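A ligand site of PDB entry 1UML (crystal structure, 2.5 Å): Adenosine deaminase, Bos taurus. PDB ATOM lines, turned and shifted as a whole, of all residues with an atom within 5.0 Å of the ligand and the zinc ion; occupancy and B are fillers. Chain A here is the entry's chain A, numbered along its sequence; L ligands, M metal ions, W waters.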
ATOM      1  N   HIS A  14     -11.621 -30.537  -0.880  1.00  0.00           N
ATOM      2  CA  HIS A  14     -11.809 -29.648  -2.014  1.00  0.00           C
ATOM      3  C   HIS A  14     -12.594 -30.302  -3.152  1.00  0.00           C
ATOM      4  O   HIS A  14     -12.080 -30.879  -4.104  1.00  0.00           O
ATOM      5  CB  HIS A  14     -10.450 -29.027  -2.417  1.00  0.00           C
ATOM      6  CG  HIS A  14     -10.590 -27.905  -3.438  1.00  0.00           C
ATOM      7  ND1 HIS A  14     -10.072 -26.677  -3.271  1.00  0.00           N
ATOM      8  CD2 HIS A  14     -11.265 -27.914  -4.654  1.00  0.00           C
ATOM      9  CE1 HIS A  14     -10.412 -25.903  -4.333  1.00  0.00           C
ATOM     10  NE2 HIS A  14     -11.150 -26.677  -5.183  1.00  0.00           N
ATOM     11  N   HIS A  16     -16.472 -29.541  -5.377  1.00  0.00           N
ATOM     12  CA  HIS A  16     -17.653 -28.723  -5.641  1.00  0.00           C
ATOM     13  C   HIS A  16     -18.881 -29.567  -5.847  1.00  0.00           C
ATOM     14  O   HIS A  16     -18.914 -30.468  -6.676  1.00  0.00           O
ATOM     15  CB  HIS A  16     -17.450 -27.867  -6.877  1.00  0.00           C
ATOM     16  CG  HIS A  16     -16.395 -26.796  -6.709  1.00  0.00           C
ATOM     17  ND1 HIS A  16     -16.676 -25.528  -6.450  1.00  0.00           N
ATOM     18  CD2 HIS A  16     -15.019 -26.902  -6.913  1.00  0.00           C
ATOM     19  CE1 HIS A  16     -15.507 -24.824  -6.491  1.00  0.00           C
ATOM     20  NE2 HIS A  16     -14.494 -25.667  -6.778  1.00  0.00           N
ATOM     21  N   ASP A  18     -21.860 -28.584  -7.056  1.00  0.00           N
ATOM     22  CA  ASP A  18     -22.374 -28.373  -8.419  1.00  0.00           C
ATOM     23  C   ASP A  18     -21.527 -28.955  -9.531  1.00  0.00           C
ATOM     24  O   ASP A  18     -21.882 -28.917 -10.695  1.00  0.00           O
ATOM     25  CB  ASP A  18     -22.713 -26.882  -8.651  1.00  0.00           C
ATOM     26  CG  ASP A  18     -21.563 -25.889  -8.458  1.00  0.00           C
ATOM     27  OD1 ASP A  18     -21.755 -24.725  -8.748  1.00  0.00           O
ATOM     28  OD2 ASP A  18     -20.485 -26.258  -8.011  1.00  0.00           O
ATOM     29  N   GLY A  19     -20.378 -29.512  -9.124  1.00  0.00           N
ATOM     30  CA  GLY A  19     -19.609 -30.277 -10.103  1.00  0.00           C
ATOM     31  C   GLY A  19     -19.516 -31.749  -9.748  1.00  0.00           C
ATOM     32  O   GLY A  19     -18.560 -32.432 -10.123  1.00  0.00           O
ATOM     33  N   LEU A  55      -9.496 -27.211 -21.911  1.00  0.00           N
ATOM     34  CA  LEU A  55     -10.384 -26.271 -22.613  1.00  0.00           C
ATOM     35  C   LEU A  55     -10.221 -24.869 -22.053  1.00  0.00           C
ATOM     36  O   LEU A  55      -9.739 -24.713 -20.938  1.00  0.00           O
ATOM     37  CB  LEU A  55     -11.869 -26.623 -22.417  1.00  0.00           C
ATOM     38  CG  LEU A  55     -12.397 -27.917 -23.058  1.00  0.00           C
ATOM     39  CD1 LEU A  55     -13.863 -28.054 -22.694  1.00  0.00           C
ATOM     40  CD2 LEU A  55     -12.220 -28.015 -24.566  1.00  0.00           C
ATOM     41  N   THR A  56     -10.686 -23.889 -22.867  1.00  0.00           N
ATOM     42  CA  THR A  56     -10.813 -22.504 -22.393  1.00  0.00           C
ATOM     43  C   THR A  56     -11.909 -22.347 -21.371  1.00  0.00           C
ATOM     44  O   THR A  56     -12.735 -23.247 -21.212  1.00  0.00           O
ATOM     45  CB  THR A  56     -11.102 -21.512 -23.538  1.00  0.00           C
ATOM     46  OG1 THR A  56     -12.435 -21.698 -24.024  1.00  0.00           O
ATOM     47  CG2 THR A  56     -10.098 -21.582 -24.688  1.00  0.00           C
ATOM     48  N   LEU A  57     -11.919 -21.150 -20.743  1.00  0.00           N
ATOM     49  CA  LEU A  57     -12.952 -20.846 -19.751  1.00  0.00           C
ATOM     50  C   LEU A  57     -14.408 -20.774 -20.230  1.00  0.00           C
ATOM     51  O   LEU A  57     -15.284 -21.336 -19.591  1.00  0.00           O
ATOM     52  CB  LEU A  57     -12.504 -19.634 -18.906  1.00  0.00           C
ATOM     53  CG  LEU A  57     -13.443 -19.152 -17.785  1.00  0.00           C
ATOM     54  CD1 LEU A  57     -13.776 -20.214 -16.725  1.00  0.00           C
ATOM     55  CD2 LEU A  57     -12.908 -17.872 -17.136  1.00  0.00           C
ATOM     56  N   PHE A  60     -15.497 -24.205 -20.771  1.00  0.00           N
ATOM     57  CA  PHE A  60     -15.757 -24.700 -19.410  1.00  0.00           C
ATOM     58  C   PHE A  60     -17.107 -24.315 -18.809  1.00  0.00           C
ATOM     59  O   PHE A  60     -17.838 -25.158 -18.326  1.00  0.00           O
ATOM     60  CB  PHE A  60     -14.578 -24.270 -18.494  1.00  0.00           C
ATOM     61  CG  PHE A  60     -14.686 -24.770 -17.062  1.00  0.00           C
ATOM     62  CD1 PHE A  60     -14.585 -26.158 -16.794  1.00  0.00           C
ATOM     63  CD2 PHE A  60     -14.896 -23.840 -16.028  1.00  0.00           C
ATOM     64  CE1 PHE A  60     -14.674 -26.613 -15.464  1.00  0.00           C
ATOM     65  CE2 PHE A  60     -14.983 -24.296 -14.688  1.00  0.00           C
ATOM     66  CZ  PHE A  60     -14.845 -25.679 -14.417  1.00  0.00           C
ATOM     67  N   LEU A  61     -17.416 -22.992 -18.867  1.00  0.00           N
ATOM     68  CA  LEU A  61     -18.644 -22.487 -18.238  1.00  0.00           C
ATOM     69  C   LEU A  61     -19.957 -22.950 -18.843  1.00  0.00           C
ATOM     70  O   LEU A  61     -20.957 -23.131 -18.157  1.00  0.00           O
ATOM     71  CB  LEU A  61     -18.680 -20.950 -18.199  1.00  0.00           C
ATOM     72  CG  LEU A  61     -17.621 -20.307 -17.312  1.00  0.00           C
ATOM     73  CD1 LEU A  61     -17.700 -18.784 -17.378  1.00  0.00           C
ATOM     74  CD2 LEU A  61     -17.675 -20.844 -15.863  1.00  0.00           C
ATOM     75  N   PHE A  64     -21.610 -25.915 -17.388  1.00  0.00           N
ATOM     76  CA  PHE A  64     -22.628 -25.618 -16.369  1.00  0.00           C
ATOM     77  C   PHE A  64     -23.965 -25.194 -16.964  1.00  0.00           C
ATOM     78  O   PHE A  64     -25.024 -25.603 -16.490  1.00  0.00           O
ATOM     79  CB  PHE A  64     -22.176 -24.517 -15.381  1.00  0.00           C
ATOM     80  CG  PHE A  64     -20.962 -24.881 -14.572  1.00  0.00           C
ATOM     81  CD1 PHE A  64     -19.702 -24.401 -14.967  1.00  0.00           C
ATOM     82  CD2 PHE A  64     -21.097 -25.692 -13.428  1.00  0.00           C
ATOM     83  CE1 PHE A  64     -18.554 -24.767 -14.237  1.00  0.00           C
ATOM     84  CE2 PHE A  64     -19.959 -26.064 -12.685  1.00  0.00           C
ATOM     85  CZ  PHE A  64     -18.694 -25.620 -13.126  1.00  0.00           C
ATOM     86  N   ARG A 100     -18.024 -27.895  -1.185  1.00  0.00           N
ATOM     87  CA  ARG A 100     -18.285 -26.475  -1.377  1.00  0.00           C
ATOM     88  C   ARG A 100     -19.229 -26.166  -2.512  1.00  0.00           C
ATOM     89  O   ARG A 100     -19.314 -26.866  -3.528  1.00  0.00           O
ATOM     90  CB  ARG A 100     -16.965 -25.699  -1.503  1.00  0.00           C
ATOM     91  CG  ARG A 100     -16.246 -25.890  -2.842  1.00  0.00           C
ATOM     92  CD  ARG A 100     -14.762 -26.166  -2.683  1.00  0.00           C
ATOM     93  NE  ARG A 100     -14.057 -25.057  -2.073  1.00  0.00           N
ATOM     94  CZ  ARG A 100     -12.904 -25.215  -1.407  1.00  0.00           C
ATOM     95  NH1 ARG A 100     -12.024 -24.240  -1.448  1.00  0.00           N
ATOM     96  NH2 ARG A 100     -12.621 -26.320  -0.721  1.00  0.00           N
ATOM     97  N   TYR A 101     -19.926 -25.054  -2.295  1.00  0.00           N
ATOM     98  CA  TYR A 101     -20.787 -24.596  -3.382  1.00  0.00           C
ATOM     99  C   TYR A 101     -21.187 -23.161  -3.146  1.00  0.00           C
ATOM    100  O   TYR A 101     -21.082 -22.624  -2.046  1.00  0.00           O
ATOM    101  CB  TYR A 101     -22.044 -25.504  -3.577  1.00  0.00           C
ATOM    102  CG  TYR A 101     -22.943 -25.484  -2.361  1.00  0.00           C
ATOM    103  CD1 TYR A 101     -24.090 -24.691  -2.389  1.00  0.00           C
ATOM    104  CD2 TYR A 101     -22.577 -26.225  -1.209  1.00  0.00           C
ATOM    105  CE1 TYR A 101     -24.881 -24.579  -1.237  1.00  0.00           C
ATOM    106  CE2 TYR A 101     -23.348 -26.100  -0.050  1.00  0.00           C
ATOM    107  CZ  TYR A 101     -24.502 -25.293  -0.086  1.00  0.00           C
ATOM    108  OH  TYR A 101     -25.293 -25.192   1.044  1.00  0.00           O
ATOM    109  N   SER A 102     -21.691 -22.586  -4.254  1.00  0.00           N
ATOM    110  CA  SER A 102     -22.375 -21.304  -4.138  1.00  0.00           C
ATOM    111  C   SER A 102     -23.890 -21.442  -4.071  1.00  0.00           C
ATOM    112  O   SER A 102     -24.548 -21.835  -5.017  1.00  0.00           O
ATOM    113  CB  SER A 102     -22.014 -20.467  -5.335  1.00  0.00           C
ATOM    114  OG  SER A 102     -22.914 -19.371  -5.366  1.00  0.00           O
ATOM    115  N   LEU A 105     -26.065 -19.605  -6.790  1.00  0.00           N
ATOM    116  CA  LEU A 105     -26.103 -20.308  -8.083  1.00  0.00           C
ATOM    117  C   LEU A 105     -27.053 -21.473  -8.188  1.00  0.00           C
ATOM    118  O   LEU A 105     -27.241 -22.025  -9.273  1.00  0.00           O
ATOM    119  CB  LEU A 105     -24.731 -20.803  -8.514  1.00  0.00           C
ATOM    120  CG  LEU A 105     -23.687 -19.708  -8.680  1.00  0.00           C
ATOM    121  CD1 LEU A 105     -22.432 -20.259  -9.338  1.00  0.00           C
ATOM    122  CD2 LEU A 105     -24.226 -18.503  -9.449  1.00  0.00           C
ATOM    123  N   CYS A 152     -19.210 -20.861  -1.009  1.00  0.00           N
ATOM    124  CA  CYS A 152     -18.427 -20.025  -1.923  1.00  0.00           C
ATOM    125  C   CYS A 152     -19.008 -18.640  -2.146  1.00  0.00           C
ATOM    126  O   CYS A 152     -20.159 -18.513  -2.508  1.00  0.00           O
ATOM    127  CB  CYS A 152     -18.314 -20.679  -3.293  1.00  0.00           C
ATOM    128  SG  CYS A 152     -17.627 -22.338  -3.217  1.00  0.00           S
ATOM    129  N   MET A 154     -18.432 -15.559  -4.942  1.00  0.00           N
ATOM    130  CA  MET A 154     -18.053 -15.499  -6.354  1.00  0.00           C
ATOM    131  C   MET A 154     -17.275 -14.223  -6.706  1.00  0.00           C
ATOM    132  O   MET A 154     -17.694 -13.132  -6.383  1.00  0.00           O
ATOM    133  CB  MET A 154     -19.310 -15.603  -7.206  1.00  0.00           C
ATOM    134  CG  MET A 154     -20.114 -16.902  -7.055  1.00  0.00           C
ATOM    135  SD  MET A 154     -19.162 -18.382  -7.498  1.00  0.00           S
ATOM    136  CE  MET A 154     -18.514 -17.887  -9.131  1.00  0.00           C
ATOM    137  N   HIS A 156     -16.744 -12.327  -9.350  1.00  0.00           N
ATOM    138  CA  HIS A 156     -17.377 -11.311 -10.179  1.00  0.00           C
ATOM    139  C   HIS A 156     -18.546 -10.601  -9.524  1.00  0.00           C
ATOM    140  O   HIS A 156     -19.127  -9.641 -10.029  1.00  0.00           O
ATOM    141  CB  HIS A 156     -17.755 -11.875 -11.554  1.00  0.00           C
ATOM    142  CG  HIS A 156     -18.823 -12.959 -11.465  1.00  0.00           C
ATOM    143  ND1 HIS A 156     -18.665 -14.149 -10.843  1.00  0.00           N
ATOM    144  CD2 HIS A 156     -20.123 -12.896 -11.986  1.00  0.00           C
ATOM    145  CE1 HIS A 156     -19.839 -14.830 -10.963  1.00  0.00           C
ATOM    146  NE2 HIS A 156     -20.742 -14.060 -11.666  1.00  0.00           N
ATOM    147  N   ALA A 182     -14.517 -18.089  -4.997  1.00  0.00           N
ATOM    148  CA  ALA A 182     -14.378 -18.898  -6.191  1.00  0.00           C
ATOM    149  C   ALA A 182     -14.718 -18.103  -7.435  1.00  0.00           C
ATOM    150  O   ALA A 182     -15.243 -16.986  -7.366  1.00  0.00           O
ATOM    151  CB  ALA A 182     -15.280 -20.150  -6.068  1.00  0.00           C
ATOM    152  N   GLY A 183     -14.362 -18.728  -8.565  1.00  0.00           N
ATOM    153  CA  GLY A 183     -14.726 -18.266  -9.905  1.00  0.00           C
ATOM    154  C   GLY A 183     -13.997 -17.114 -10.586  1.00  0.00           C
ATOM    155  O   GLY A 183     -14.543 -16.021 -10.698  1.00  0.00           O
ATOM    156  N   ASP A 184     -12.806 -17.412 -11.127  1.00  0.00           N
ATOM    157  CA  ASP A 184     -12.098 -16.473 -12.038  1.00  0.00           C
ATOM    158  C   ASP A 184     -11.214 -15.426 -11.356  1.00  0.00           C
ATOM    159  O   ASP A 184     -11.513 -14.251 -11.224  1.00  0.00           O
ATOM    160  CB  ASP A 184     -12.948 -15.877 -13.207  1.00  0.00           C
ATOM    161  CG  ASP A 184     -12.135 -15.346 -14.420  1.00  0.00           C
ATOM    162  OD1 ASP A 184     -10.898 -15.328 -14.411  1.00  0.00           O
ATOM    163  OD2 ASP A 184     -12.754 -14.948 -15.417  1.00  0.00           O
ATOM    164  N   HIS A 213      -9.583 -19.671  -3.301  1.00  0.00           N
ATOM    165  CA  HIS A 213      -9.040 -20.297  -4.499  1.00  0.00           C
ATOM    166  C   HIS A 213      -7.750 -19.834  -5.158  1.00  0.00           C
ATOM    167  O   HIS A 213      -7.141 -20.631  -5.841  1.00  0.00           O
ATOM    168  CB  HIS A 213     -10.066 -20.347  -5.587  1.00  0.00           C
ATOM    169  CG  HIS A 213     -10.975 -21.519  -5.465  1.00  0.00           C
ATOM    170  ND1 HIS A 213     -12.156 -21.480  -4.836  1.00  0.00           N
ATOM    171  CD2 HIS A 213     -10.832 -22.746  -6.092  1.00  0.00           C
ATOM    172  CE1 HIS A 213     -12.777 -22.659  -5.059  1.00  0.00           C
ATOM    173  NE2 HIS A 213     -11.963 -23.433  -5.833  1.00  0.00           N
ATOM    174  N   GLU A 216      -4.480 -20.979  -8.976  1.00  0.00           N
ATOM    175  CA  GLU A 216      -4.530 -22.030  -9.999  1.00  0.00           C
ATOM    176  C   GLU A 216      -4.155 -21.512 -11.350  1.00  0.00           C
ATOM    177  O   GLU A 216      -3.298 -22.051 -12.040  1.00  0.00           O
ATOM    178  CB  GLU A 216      -5.842 -22.854 -10.074  1.00  0.00           C
ATOM    179  CG  GLU A 216      -7.166 -22.111 -10.214  1.00  0.00           C
ATOM    180  CD  GLU A 216      -8.366 -23.035 -10.473  1.00  0.00           C
ATOM    181  OE1 GLU A 216      -9.432 -22.764  -9.928  1.00  0.00           O
ATOM    182  OE2 GLU A 216      -8.243 -23.999 -11.237  1.00  0.00           O
ATOM    183  N   VAL A 217      -4.843 -20.420 -11.670  1.00  0.00           N
ATOM    184  CA  VAL A 217      -4.680 -19.901 -13.009  1.00  0.00           C
ATOM    185  C   VAL A 217      -4.122 -18.482 -13.007  1.00  0.00           C
ATOM    186  O   VAL A 217      -3.828 -17.912 -14.051  1.00  0.00           O
ATOM    187  CB  VAL A 217      -6.024 -20.084 -13.737  1.00  0.00           C
ATOM    188  CG1 VAL A 217      -7.060 -18.977 -13.555  1.00  0.00           C
ATOM    189  CG2 VAL A 217      -5.790 -20.453 -15.178  1.00  0.00           C
ATOM    190  N   HIS A 237      -5.689 -24.861  -4.393  1.00  0.00           N
ATOM    191  CA  HIS A 237      -4.643 -24.905  -5.426  1.00  0.00           C
ATOM    192  C   HIS A 237      -3.278 -24.324  -5.025  1.00  0.00           C
ATOM    193  O   HIS A 237      -2.371 -25.032  -4.614  1.00  0.00           O
ATOM    194  CB  HIS A 237      -5.111 -24.327  -6.766  1.00  0.00           C
ATOM    195  CG  HIS A 237      -6.361 -25.009  -7.291  1.00  0.00           C
ATOM    196  ND1 HIS A 237      -6.370 -26.185  -7.944  1.00  0.00           N
ATOM    197  CD2 HIS A 237      -7.673 -24.535  -7.221  1.00  0.00           C
ATOM    198  CE1 HIS A 237      -7.668 -26.465  -8.291  1.00  0.00           C
ATOM    199  NE2 HIS A 237      -8.457 -25.451  -7.840  1.00  0.00           N
ATOM    200  N   THR A 268      -7.782 -27.985 -16.785  1.00  0.00           N
ATOM    201  CA  THR A 268      -8.028 -26.537 -16.783  1.00  0.00           C
ATOM    202  C   THR A 268      -7.004 -25.703 -17.541  1.00  0.00           C
ATOM    203  O   THR A 268      -7.233 -24.532 -17.854  1.00  0.00           O
ATOM    204  CB  THR A 268      -8.061 -25.976 -15.366  1.00  0.00           C
ATOM    205  OG1 THR A 268      -6.793 -26.156 -14.746  1.00  0.00           O
ATOM    206  CG2 THR A 268      -9.186 -26.549 -14.514  1.00  0.00           C
ATOM    207  N   ASP A 294     -11.997 -32.032  -7.087  1.00  0.00           N
ATOM    208  CA  ASP A 294     -12.528 -30.785  -7.629  1.00  0.00           C
ATOM    209  C   ASP A 294     -13.915 -30.891  -8.220  1.00  0.00           C
ATOM    210  O   ASP A 294     -14.894 -30.527  -7.592  1.00  0.00           O
ATOM    211  CB  ASP A 294     -11.499 -30.133  -8.568  1.00  0.00           C
ATOM    212  CG  ASP A 294     -11.525 -28.612  -8.553  1.00  0.00           C
ATOM    213  OD1 ASP A 294     -10.708 -28.012  -9.228  1.00  0.00           O
ATOM    214  OD2 ASP A 294     -12.352 -28.033  -7.865  1.00  0.00           O
ATOM    215  N   ASP A 295     -13.958 -31.392  -9.463  1.00  0.00           N
ATOM    216  CA  ASP A 295     -15.235 -31.563 -10.173  1.00  0.00           C
ATOM    217  C   ASP A 295     -15.302 -32.934 -10.863  1.00  0.00           C
ATOM    218  O   ASP A 295     -14.990 -33.061 -12.042  1.00  0.00           O
ATOM    219  CB  ASP A 295     -15.478 -30.503 -11.260  1.00  0.00           C
ATOM    220  CG  ASP A 295     -15.276 -29.076 -10.777  1.00  0.00           C
ATOM    221  OD1 ASP A 295     -16.261 -28.425 -10.461  1.00  0.00           O
ATOM    222  OD2 ASP A 295     -14.140 -28.622 -10.741  1.00  0.00           O
ATOM    223  N   PHE A 299     -14.775 -33.510 -14.755  1.00  0.00           N
ATOM    224  CA  PHE A 299     -13.505 -34.144 -15.148  1.00  0.00           C
ATOM    225  C   PHE A 299     -13.531 -35.663 -15.285  1.00  0.00           C
ATOM    226  O   PHE A 299     -12.487 -36.307 -15.326  1.00  0.00           O
ATOM    227  CB  PHE A 299     -12.355 -33.711 -14.215  1.00  0.00           C
ATOM    228  CG  PHE A 299     -12.278 -32.216 -14.008  1.00  0.00           C
ATOM    229  CD1 PHE A 299     -12.401 -31.324 -15.113  1.00  0.00           C
ATOM    230  CD2 PHE A 299     -12.099 -31.724 -12.701  1.00  0.00           C
ATOM    231  CE1 PHE A 299     -12.403 -29.935 -14.879  1.00  0.00           C
ATOM    232  CE2 PHE A 299     -12.079 -30.334 -12.471  1.00  0.00           C
ATOM    233  CZ  PHE A 299     -12.259 -29.449 -13.566  1.00  0.00           C
HETATM  234  C1  LIG L   1     -16.421 -23.474  -9.793  1.00  0.00           C
HETATM  235  N1  LIG L   1     -17.756 -24.008  -9.510  1.00  0.00           N
HETATM  236  C2  LIG L   1     -17.765 -25.346  -9.655  1.00  0.00           C
HETATM  237  N2  LIG L   1     -16.545 -25.745 -10.017  1.00  0.00           N
HETATM  238  C3  LIG L   1     -15.707 -24.562 -10.123  1.00  0.00           C
HETATM  239  C4  LIG L   1     -14.289 -24.568 -10.542  1.00  0.00           C
HETATM  240  O1  LIG L   1     -13.771 -23.499 -10.809  1.00  0.00           O
HETATM  241  N3  LIG L   1     -13.639 -25.723 -10.630  1.00  0.00           N
HETATM  242  C5  LIG L   1     -18.917 -23.226  -9.106  1.00  0.00           C
HETATM  243  C6  LIG L   1     -18.951 -23.030  -7.577  1.00  0.00           C
HETATM  244  O2  LIG L   1     -18.954 -24.241  -6.873  1.00  0.00           O
HETATM  245  C7  LIG L   1     -19.029 -21.893  -9.868  1.00  0.00           C
HETATM  246  C8  LIG L   1     -18.911 -22.008 -11.396  1.00  0.00           C
HETATM  247  N4  LIG L   1     -18.593 -20.702 -11.971  1.00  0.00           N
HETATM  248  C9  LIG L   1     -19.442 -19.655 -12.211  1.00  0.00           C
HETATM  249  C10 LIG L   1     -18.729 -18.571 -12.730  1.00  0.00           C
HETATM  250  C11 LIG L   1     -17.360 -18.994 -12.807  1.00  0.00           C
HETATM  251  C12 LIG L   1     -17.307 -20.334 -12.320  1.00  0.00           C
HETATM  252  C13 LIG L   1     -16.219 -18.369 -13.227  1.00  0.00           C
HETATM  253  C14 LIG L   1     -15.007 -19.060 -13.183  1.00  0.00           C
HETATM  254  C15 LIG L   1     -14.946 -20.382 -12.697  1.00  0.00           C
HETATM  255  C16 LIG L   1     -16.118 -21.003 -12.269  1.00  0.00           C
HETATM  256  N5  LIG L   1     -13.783 -21.082 -12.602  1.00  0.00           N
HETATM  257  C17 LIG L   1     -12.569 -20.691 -13.058  1.00  0.00           C
HETATM  258  O3  LIG L   1     -12.321 -19.652 -13.672  1.00  0.00           O
HETATM  259  C18 LIG L   1     -11.502 -21.720 -12.707  1.00  0.00           C
HETATM  260  C19 LIG L   1     -10.252 -21.562 -13.579  1.00  0.00           C
HETATM  261  C20 LIG L   1     -11.114 -23.315 -15.197  1.00  0.00           C
HETATM  262  C21 LIG L   1     -10.448 -22.113 -14.980  1.00  0.00           C
HETATM  263  C22 LIG L   1      -9.910 -21.416 -16.061  1.00  0.00           C
HETATM  264  C23 LIG L   1     -10.020 -21.940 -17.344  1.00  0.00           C
HETATM  265  C24 LIG L   1     -10.655 -23.157 -17.548  1.00  0.00           C
HETATM  266  C25 LIG L   1     -11.204 -23.849 -16.474  1.00  0.00           C
HETATM  267 ZN    ZN M   1     -12.314 -25.625  -6.864  1.00  0.00          ZN
HETATM  268  O   HOH W   1     -11.371 -24.642  -8.811  1.00  0.00           O
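Merely in contact with the ligand: Gly 183 (3.4 Å), Leu 57 (3.4 Å), Leu 61 (3.6 Å), Phe 64 (3.6 Å), Glu 216 (3.6 Å), Phe 60 (3.6 Å), Met 154 (3.7 Å), Thr 268 (3.7 Å), Leu 105 (3.8 Å), Leu 55 (3.8 Å) and Tyr 101 (3.96 Å). Hydrophobic or aromatic side chains that line the ligand: His 16, Leu 57, Phe 60, Leu 61, Phe 64, Leu 105 and Met 154. 16 residues have an atom within 4 Å of the ligand: His 16, Asp 18, Leu 55, Leu 57, Phe 60, Leu 61, Phe 64, Tyr 101, Leu 105, Met 154, Gly 183, Asp 184, Glu 216, Thr 268, Asp 294 and Asp 295. The nearest printed residue that does not touch the ligand is Thr 56 (4.1 Å).
Water W1 lies within hydrogen-bond range of OE1 of Glu 216, N3 of the ligand, NE2 of His 237 and OD1 of Asp 294.
A ring nitrogen (ND1) of His 16 is in hydrogen-bond range of an oxygen (O2) of the ligand, 2.7 Å away. The side-chain carboxylate (OD1) of Asp 295 sits at hydrogen-bond distance from a nitrogen (N2) of the ligand (2.7 Å). OD2 of Asp 18 sits at hydrogen-bond distance from O2 of the ligand, 2.8 Å away. N of Asp 184 lies within hydrogen-bond range of O3 of the ligand, 3.4 Å away.
N of Leu 105 sits close to OG of Ser 102. The backbone NH (N) of Cys 152 is in hydrogen-bond range of the backbone carbonyl oxygen (O) of Tyr 101 (2.8 Å).
Residues that only touch the zinc ion: His 237 (3.98 Å). Within 4 Å of the zinc ion: His 14, His 16, His 213, His 237 and Asp 294. The nearest printed residue that does not touch the zinc ion is Arg 100 (4.9 Å).
NE2 of His 16 binds the zinc ion, 2.2 Å away. The zinc ion is bound by a ring nitrogen (NE2) of His 14, 2.3 Å away. Water W1 is bound to the zinc ion (2.4 Å). The zinc ion is bound by a ring nitrogen (NE2) of His 213, 2.4 Å away. OD2 of Asp 294 is bound to the zinc ion, 2.6 Å away.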
